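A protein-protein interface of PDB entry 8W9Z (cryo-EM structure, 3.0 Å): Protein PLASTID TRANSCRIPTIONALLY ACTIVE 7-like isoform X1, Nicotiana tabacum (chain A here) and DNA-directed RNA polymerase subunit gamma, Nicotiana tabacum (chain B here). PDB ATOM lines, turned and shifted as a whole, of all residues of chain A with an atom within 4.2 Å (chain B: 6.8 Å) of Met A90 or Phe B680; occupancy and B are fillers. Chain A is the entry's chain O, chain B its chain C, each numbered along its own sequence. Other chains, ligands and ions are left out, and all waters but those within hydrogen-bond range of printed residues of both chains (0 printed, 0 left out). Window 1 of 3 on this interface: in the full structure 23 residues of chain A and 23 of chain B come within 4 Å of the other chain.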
ATOM      1  N   LYS A  86      -3.386 -17.351 -21.573  1.00  0.00           N
ATOM      2  CA  LYS A  86      -3.848 -16.042 -21.132  1.00  0.00           C
ATOM      3  C   LYS A  86      -5.110 -15.588 -21.850  1.00  0.00           C
ATOM      4  O   LYS A  86      -5.678 -14.555 -21.477  1.00  0.00           O
ATOM      5  CB  LYS A  86      -2.745 -14.997 -21.325  1.00  0.00           C
ATOM      6  CG  LYS A  86      -1.495 -15.254 -20.499  1.00  0.00           C
ATOM      7  CD  LYS A  86      -0.475 -14.143 -20.676  1.00  0.00           C
ATOM      8  CE  LYS A  86      -1.030 -12.806 -20.217  1.00  0.00           C
ATOM      9  NZ  LYS A  86      -1.408 -12.827 -18.777  1.00  0.00           N
ATOM     10  N   LEU A  87      -5.560 -16.328 -22.867  1.00  0.00           N
ATOM     11  CA  LEU A  87      -6.799 -15.974 -23.551  1.00  0.00           C
ATOM     12  C   LEU A  87      -8.008 -16.137 -22.638  1.00  0.00           C
ATOM     13  O   LEU A  87      -8.964 -15.358 -22.733  1.00  0.00           O
ATOM     14  CB  LEU A  87      -6.970 -16.829 -24.805  1.00  0.00           C
ATOM     15  CG  LEU A  87      -5.817 -16.851 -25.809  1.00  0.00           C
ATOM     16  CD1 LEU A  87      -6.123 -17.810 -26.948  1.00  0.00           C
ATOM     17  CD2 LEU A  87      -5.534 -15.458 -26.342  1.00  0.00           C
ATOM     18  N   LEU A  88      -7.983 -17.136 -21.754  1.00  0.00           N
ATOM     19  CA  LEU A  88      -9.112 -17.363 -20.858  1.00  0.00           C
ATOM     20  C   LEU A  88      -9.245 -16.237 -19.841  1.00  0.00           C
ATOM     21  O   LEU A  88     -10.363 -15.855 -19.472  1.00  0.00           O
ATOM     22  CB  LEU A  88      -8.953 -18.711 -20.157  1.00  0.00           C
ATOM     23  CG  LEU A  88     -10.136 -19.200 -19.324  1.00  0.00           C
ATOM     24  CD1 LEU A  88     -11.371 -19.338 -20.194  1.00  0.00           C
ATOM     25  CD2 LEU A  88      -9.798 -20.518 -18.651  1.00  0.00           C
ATOM     26  N   THR A  89      -8.117 -15.695 -19.376  1.00  0.00           N
ATOM     27  CA  THR A  89      -8.163 -14.581 -18.435  1.00  0.00           C
ATOM     28  C   THR A  89      -8.787 -13.344 -19.065  1.00  0.00           C
ATOM     29  O   THR A  89      -9.417 -12.542 -18.367  1.00  0.00           O
ATOM     30  CB  THR A  89      -6.757 -14.263 -17.925  1.00  0.00           C
ATOM     31  OG1 THR A  89      -5.944 -13.811 -19.015  1.00  0.00           O
ATOM     32  CG2 THR A  89      -6.124 -15.500 -17.309  1.00  0.00           C
ATOM     33  N   MET A  90      -8.625 -13.172 -20.378  1.00  0.00           N
ATOM     34  CA  MET A  90      -9.279 -12.068 -21.068  1.00  0.00           C
ATOM     35  C   MET A  90     -10.745 -12.374 -21.339  1.00  0.00           C
ATOM     36  O   MET A  90     -11.598 -11.484 -21.234  1.00  0.00           O
ATOM     37  CB  MET A  90      -8.559 -11.763 -22.381  1.00  0.00           C
ATOM     38  CG  MET A  90      -7.048 -11.783 -22.286  1.00  0.00           C
ATOM     39  SD  MET A  90      -6.272 -11.390 -23.865  1.00  0.00           S
ATOM     40  CE  MET A  90      -7.141 -12.518 -24.948  1.00  0.00           C
ATOM     41  N   ASP A  91     -11.054 -13.624 -21.689  1.00  0.00           N
ATOM     42  CA  ASP A  91     -12.431 -13.984 -22.009  1.00  0.00           C
ATOM     43  C   ASP A  91     -13.330 -13.891 -20.783  1.00  0.00           C
ATOM     44  O   ASP A  91     -14.481 -13.450 -20.887  1.00  0.00           O
ATOM     45  CB  ASP A  91     -12.480 -15.389 -22.607  1.00  0.00           C
ATOM     46  CG  ASP A  91     -11.794 -15.469 -23.955  1.00  0.00           C
ATOM     47  OD1 ASP A  91     -11.288 -14.430 -24.428  1.00  0.00           O
ATOM     48  OD2 ASP A  91     -11.760 -16.570 -24.544  1.00  0.00           O
ATOM     49  N   ILE A  92     -12.829 -14.296 -19.614  1.00  0.00           N
ATOM     50  CA  ILE A  92     -13.626 -14.199 -18.394  1.00  0.00           C
ATOM     51  C   ILE A  92     -13.931 -12.741 -18.075  1.00  0.00           C
ATOM     52  O   ILE A  92     -15.067 -12.380 -17.739  1.00  0.00           O
ATOM     53  CB  ILE A  92     -12.908 -14.895 -17.225  1.00  0.00           C
ATOM     54  CG1 ILE A  92     -12.821 -16.402 -17.473  1.00  0.00           C
ATOM     55  CG2 ILE A  92     -13.619 -14.610 -15.914  1.00  0.00           C
ATOM     56  CD1 ILE A  92     -12.114 -17.162 -16.372  1.00  0.00           C
ATOM     57  N   HIS A  93     -12.920 -11.876 -18.185  1.00  0.00           N
ATOM     58  CA  HIS A  93     -13.122 -10.460 -17.905  1.00  0.00           C
ATOM     59  C   HIS A  93     -14.048  -9.813 -18.927  1.00  0.00           C
ATOM     60  O   HIS A  93     -14.796  -8.891 -18.584  1.00  0.00           O
ATOM     61  CB  HIS A  93     -11.779  -9.734 -17.868  1.00  0.00           C
ATOM     62  CG  HIS A  93     -11.885  -8.286 -17.503  1.00  0.00           C
ATOM     63  ND1 HIS A  93     -11.999  -7.287 -18.445  1.00  0.00           N
ATOM     64  CD2 HIS A  93     -11.892  -7.669 -16.297  1.00  0.00           C
ATOM     65  CE1 HIS A  93     -12.072  -6.117 -17.836  1.00  0.00           C
ATOM     66  NE2 HIS A  93     -12.010  -6.321 -16.532  1.00  0.00           N
ATOM     67  N   ARG A  94     -14.015 -10.275 -20.179  1.00  0.00           N
ATOM     68  CA  ARG A  94     -14.923  -9.734 -21.183  1.00  0.00           C
ATOM     69  C   ARG A  94     -16.355 -10.187 -20.931  1.00  0.00           C
ATOM     70  O   ARG A  94     -17.298  -9.410 -21.112  1.00  0.00           O
ATOM     71  CB  ARG A  94     -14.462 -10.142 -22.583  1.00  0.00           C
ATOM     72  N   ARG A 145     -12.464 -19.030 -30.951  1.00  0.00           N
ATOM     73  CA  ARG A 145     -11.673 -19.631 -29.890  1.00  0.00           C
ATOM     74  C   ARG A 145     -11.568 -21.131 -30.123  1.00  0.00           C
ATOM     75  O   ARG A 145     -12.424 -21.736 -30.775  1.00  0.00           O
ATOM     76  CB  ARG A 145     -12.280 -19.357 -28.508  1.00  0.00           C
ATOM     77  CG  ARG A 145     -12.089 -17.933 -28.017  1.00  0.00           C
ATOM     78  CD  ARG A 145     -10.628 -17.654 -27.703  1.00  0.00           C
ATOM     79  NE  ARG A 145     -10.428 -16.313 -27.165  1.00  0.00           N
ATOM     80  CZ  ARG A 145     -10.045 -15.267 -27.888  1.00  0.00           C
ATOM     81  NH1 ARG A 145      -9.815 -15.405 -29.186  1.00  0.00           N
ATOM     82  NH2 ARG A 145      -9.889 -14.083 -27.313  1.00  0.00           N
ATOM     83  N   HIS B 523      -5.580 -12.484 -11.283  1.00  0.00           N
ATOM     84  CA  HIS B 523      -5.813 -11.365 -12.186  1.00  0.00           C
ATOM     85  C   HIS B 523      -7.145 -10.669 -11.939  1.00  0.00           C
ATOM     86  O   HIS B 523      -7.410  -9.637 -12.565  1.00  0.00           O
ATOM     87  CB  HIS B 523      -5.736 -11.833 -13.641  1.00  0.00           C
ATOM     88  CG  HIS B 523      -6.833 -12.773 -14.035  1.00  0.00           C
ATOM     89  ND1 HIS B 523      -6.705 -14.142 -13.950  1.00  0.00           N
ATOM     90  CD2 HIS B 523      -8.073 -12.540 -14.524  1.00  0.00           C
ATOM     91  CE1 HIS B 523      -7.822 -14.712 -14.366  1.00  0.00           C
ATOM     92  NE2 HIS B 523      -8.669 -13.763 -14.719  1.00  0.00           N
ATOM     93  N   GLU B 675       4.312  -1.870 -26.743  1.00  0.00           N
ATOM     94  CA  GLU B 675       4.226  -3.130 -27.467  1.00  0.00           C
ATOM     95  C   GLU B 675       3.468  -4.181 -26.669  1.00  0.00           C
ATOM     96  O   GLU B 675       2.775  -5.012 -27.260  1.00  0.00           O
ATOM     97  CB  GLU B 675       5.626  -3.627 -27.838  1.00  0.00           C
ATOM     98  N   ALA B 676       3.553  -4.146 -25.337  1.00  0.00           N
ATOM     99  CA  ALA B 676       2.728  -5.037 -24.529  1.00  0.00           C
ATOM    100  C   ALA B 676       1.249  -4.725 -24.720  1.00  0.00           C
ATOM    101  O   ALA B 676       0.428  -5.633 -24.906  1.00  0.00           O
ATOM    102  CB  ALA B 676       3.120  -4.925 -23.056  1.00  0.00           C
ATOM    103  N   ILE B 677       0.896  -3.438 -24.695  1.00  0.00           N
ATOM    104  CA  ILE B 677      -0.497  -3.043 -24.904  1.00  0.00           C
ATOM    105  C   ILE B 677      -0.979  -3.497 -26.279  1.00  0.00           C
ATOM    106  O   ILE B 677      -2.069  -4.068 -26.420  1.00  0.00           O
ATOM    107  CB  ILE B 677      -0.659  -1.523 -24.726  1.00  0.00           C
ATOM    108  CG1 ILE B 677      -0.376  -1.122 -23.278  1.00  0.00           C
ATOM    109  CG2 ILE B 677      -2.053  -1.081 -25.141  1.00  0.00           C
ATOM    110  CD1 ILE B 677      -0.513   0.361 -23.019  1.00  0.00           C
ATOM    111  N   GLN B 678      -0.168  -3.254 -27.312  1.00  0.00           N
ATOM    112  CA  GLN B 678      -0.584  -3.596 -28.669  1.00  0.00           C
ATOM    113  C   GLN B 678      -0.686  -5.104 -28.861  1.00  0.00           C
ATOM    114  O   GLN B 678      -1.612  -5.588 -29.524  1.00  0.00           O
ATOM    115  CB  GLN B 678       0.382  -2.988 -29.685  1.00  0.00           C
ATOM    116  CG  GLN B 678      -0.026  -3.217 -31.130  1.00  0.00           C
ATOM    117  CD  GLN B 678       0.851  -2.467 -32.109  1.00  0.00           C
ATOM    118  OE1 GLN B 678       1.679  -1.647 -31.716  1.00  0.00           O
ATOM    119  NE2 GLN B 678       0.674  -2.745 -33.395  1.00  0.00           N
ATOM    120  N   GLY B 679       0.247  -5.866 -28.289  1.00  0.00           N
ATOM    121  CA  GLY B 679       0.172  -7.311 -28.398  1.00  0.00           C
ATOM    122  C   GLY B 679      -1.022  -7.886 -27.666  1.00  0.00           C
ATOM    123  O   GLY B 679      -1.648  -8.838 -28.136  1.00  0.00           O
ATOM    124  N   PHE B 680      -1.363  -7.312 -26.509  1.00  0.00           N
ATOM    125  CA  PHE B 680      -2.572  -7.731 -25.808  1.00  0.00           C
ATOM    126  C   PHE B 680      -3.809  -7.445 -26.648  1.00  0.00           C
ATOM    127  O   PHE B 680      -4.690  -8.304 -26.796  1.00  0.00           O
ATOM    128  CB  PHE B 680      -2.656  -7.020 -24.457  1.00  0.00           C
ATOM    129  CG  PHE B 680      -3.546  -7.705 -23.463  1.00  0.00           C
ATOM    130  CD1 PHE B 680      -4.897  -7.409 -23.401  1.00  0.00           C
ATOM    131  CD2 PHE B 680      -3.029  -8.634 -22.577  1.00  0.00           C
ATOM    132  CE1 PHE B 680      -5.715  -8.033 -22.480  1.00  0.00           C
ATOM    133  CE2 PHE B 680      -3.841  -9.262 -21.655  1.00  0.00           C
ATOM    134  CZ  PHE B 680      -5.185  -8.960 -21.606  1.00  0.00           C
ATOM    135  N   SER B 681      -3.885  -6.241 -27.222  1.00  0.00           N
ATOM    136  CA  SER B 681      -5.034  -5.883 -28.048  1.00  0.00           C
ATOM    137  C   SER B 681      -5.143  -6.768 -29.283  1.00  0.00           C
ATOM    138  O   SER B 681      -6.255  -7.080 -29.725  1.00  0.00           O
ATOM    139  CB  SER B 681      -4.950  -4.413 -28.457  1.00  0.00           C
ATOM    140  OG  SER B 681      -4.944  -3.567 -27.320  1.00  0.00           O
ATOM    141  N   ARG B 682      -4.010  -7.181 -29.855  1.00  0.00           N
ATOM    142  CA  ARG B 682      -4.054  -8.022 -31.045  1.00  0.00           C
ATOM    143  C   ARG B 682      -4.395  -9.468 -30.704  1.00  0.00           C
ATOM    144  O   ARG B 682      -5.188 -10.102 -31.409  1.00  0.00           O
ATOM    145  CB  ARG B 682      -2.724  -7.948 -31.797  1.00  0.00           C
ATOM    146  CG  ARG B 682      -2.679  -8.814 -33.044  1.00  0.00           C
ATOM    147  CD  ARG B 682      -1.652  -8.307 -34.043  1.00  0.00           C
ATOM    148  NE  ARG B 682      -0.304  -8.278 -33.487  1.00  0.00           N
ATOM    149  CZ  ARG B 682       0.773  -7.892 -34.164  1.00  0.00           C
ATOM    150  NH1 ARG B 682       0.659  -7.499 -35.426  1.00  0.00           N
ATOM    151  NH2 ARG B 682       1.963  -7.896 -33.581  1.00  0.00           N
ATOM    152  N   ALA B 683      -3.810 -10.009 -29.631  1.00  0.00           N
ATOM    153  CA  ALA B 683      -4.140 -11.361 -29.203  1.00  0.00           C
ATOM    154  C   ALA B 683      -5.571 -11.472 -28.697  1.00  0.00           C
ATOM    155  O   ALA B 683      -6.125 -12.575 -28.683  1.00  0.00           O
ATOM    156  CB  ALA B 683      -3.167 -11.824 -28.119  1.00  0.00           C
ATOM    157  N   TYR B 684      -6.176 -10.358 -28.274  1.00  0.00           N
ATOM    158  CA  TYR B 684      -7.589 -10.388 -27.909  1.00  0.00           C
ATOM    159  C   TYR B 684      -8.460 -10.741 -29.108  1.00  0.00           C
ATOM    160  O   TYR B 684      -9.503 -11.387 -28.959  1.00  0.00           O
ATOM    161  CB  TYR B 684      -8.009  -9.043 -27.316  1.00  0.00           C
ATOM    162  CG  TYR B 684      -9.501  -8.910 -27.106  1.00  0.00           C
ATOM    163  CD1 TYR B 684     -10.132  -9.549 -26.047  1.00  0.00           C
ATOM    164  CD2 TYR B 684     -10.277  -8.145 -27.966  1.00  0.00           C
ATOM    165  CE1 TYR B 684     -11.495  -9.429 -25.851  1.00  0.00           C
ATOM    166  CE2 TYR B 684     -11.640  -8.019 -27.779  1.00  0.00           C
ATOM    167  CZ  TYR B 684     -12.244  -8.664 -26.720  1.00  0.00           C
ATOM    168  OH  TYR B 684     -13.602  -8.541 -26.531  1.00  0.00           O
ATOM    169  N   SER B 685      -8.047 -10.330 -30.302  1.00  0.00           N
ATOM    170  CA  SER B 685      -8.796 -10.627 -31.517  1.00  0.00           C
ATOM    171  C   SER B 685      -8.352 -11.955 -32.121  1.00  0.00           C
ATOM    172  O   SER B 685      -7.860 -12.000 -33.248  1.00  0.00           O
ATOM    173  CB  SER B 685      -8.631  -9.501 -32.539  1.00  0.00           C
ATOM    174  OG  SER B 685      -7.271  -9.337 -32.901  1.00  0.00           O
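The guanidinium group of Arg A145 is in salt-bridge range of the side-chain carboxylate of Asp A91.
The backbone carbonyl oxygen (O) of Lys A86 is in hydrogen-bond range of the side-chain hydroxyl (OG1) of Thr A89.
CD2 of Leu A87 touches O of Ala B683, 3.8 Å away.
Thr A89 touches His B523 (CG2 to CE1, 3.5 Å).
Phe B680 touches Met A90.
Ala B683 touches Met A90 (O to CE, 3.9 Å).
CA of Tyr B684 touches CE of Met A90, at 3.7 Å.
Of the printed residues of chain B, Leu A87 touches Ala B683.
Leu A88 touches none of the printed residues of chain B.
Of the printed residues of chain B, Thr A89 touches His B523.
Of the printed residues of chain B, Met A90 touches Phe B680, Ala B683 and Tyr B684.
Of the printed residues of chain B, Arg A145 touches Tyr B684.
Of the printed residues of chain A, His B523 touches Thr A89 (3.5 Å).
Of chain A, only Met A90 (3.4 Å) comes within 4 Å of Phe B680.
Of the printed residues of chain A, Tyr B684 touches Met A90 (3.7 Å) and Arg A145 (3.2 Å).
The nearest printed residue of chain A that does not touch Phe B680 is Lys A86 (4.7 Å).
Hydrophobic or aromatic side chains of chain A that line the printed part of chain B: Leu A87 and Met A90.
Of the 12 printed residues of chain B, 4 touch a printed residue of chain A.
Hydrophobic or aromatic side chains of chain B within 4 Å of the printed part of chain A: His B523 and Phe B680.
Among the printed residues, 6 pairs touch across the chains.
Among the printed residues, no Asp or Glu carboxylate lies within 4 Å of a Lys or Arg side-chain nitrogen of the other chain.
NH2 of Arg A145 sits at hydrogen-bond distance from O of Tyr B684 (3.2 Å).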
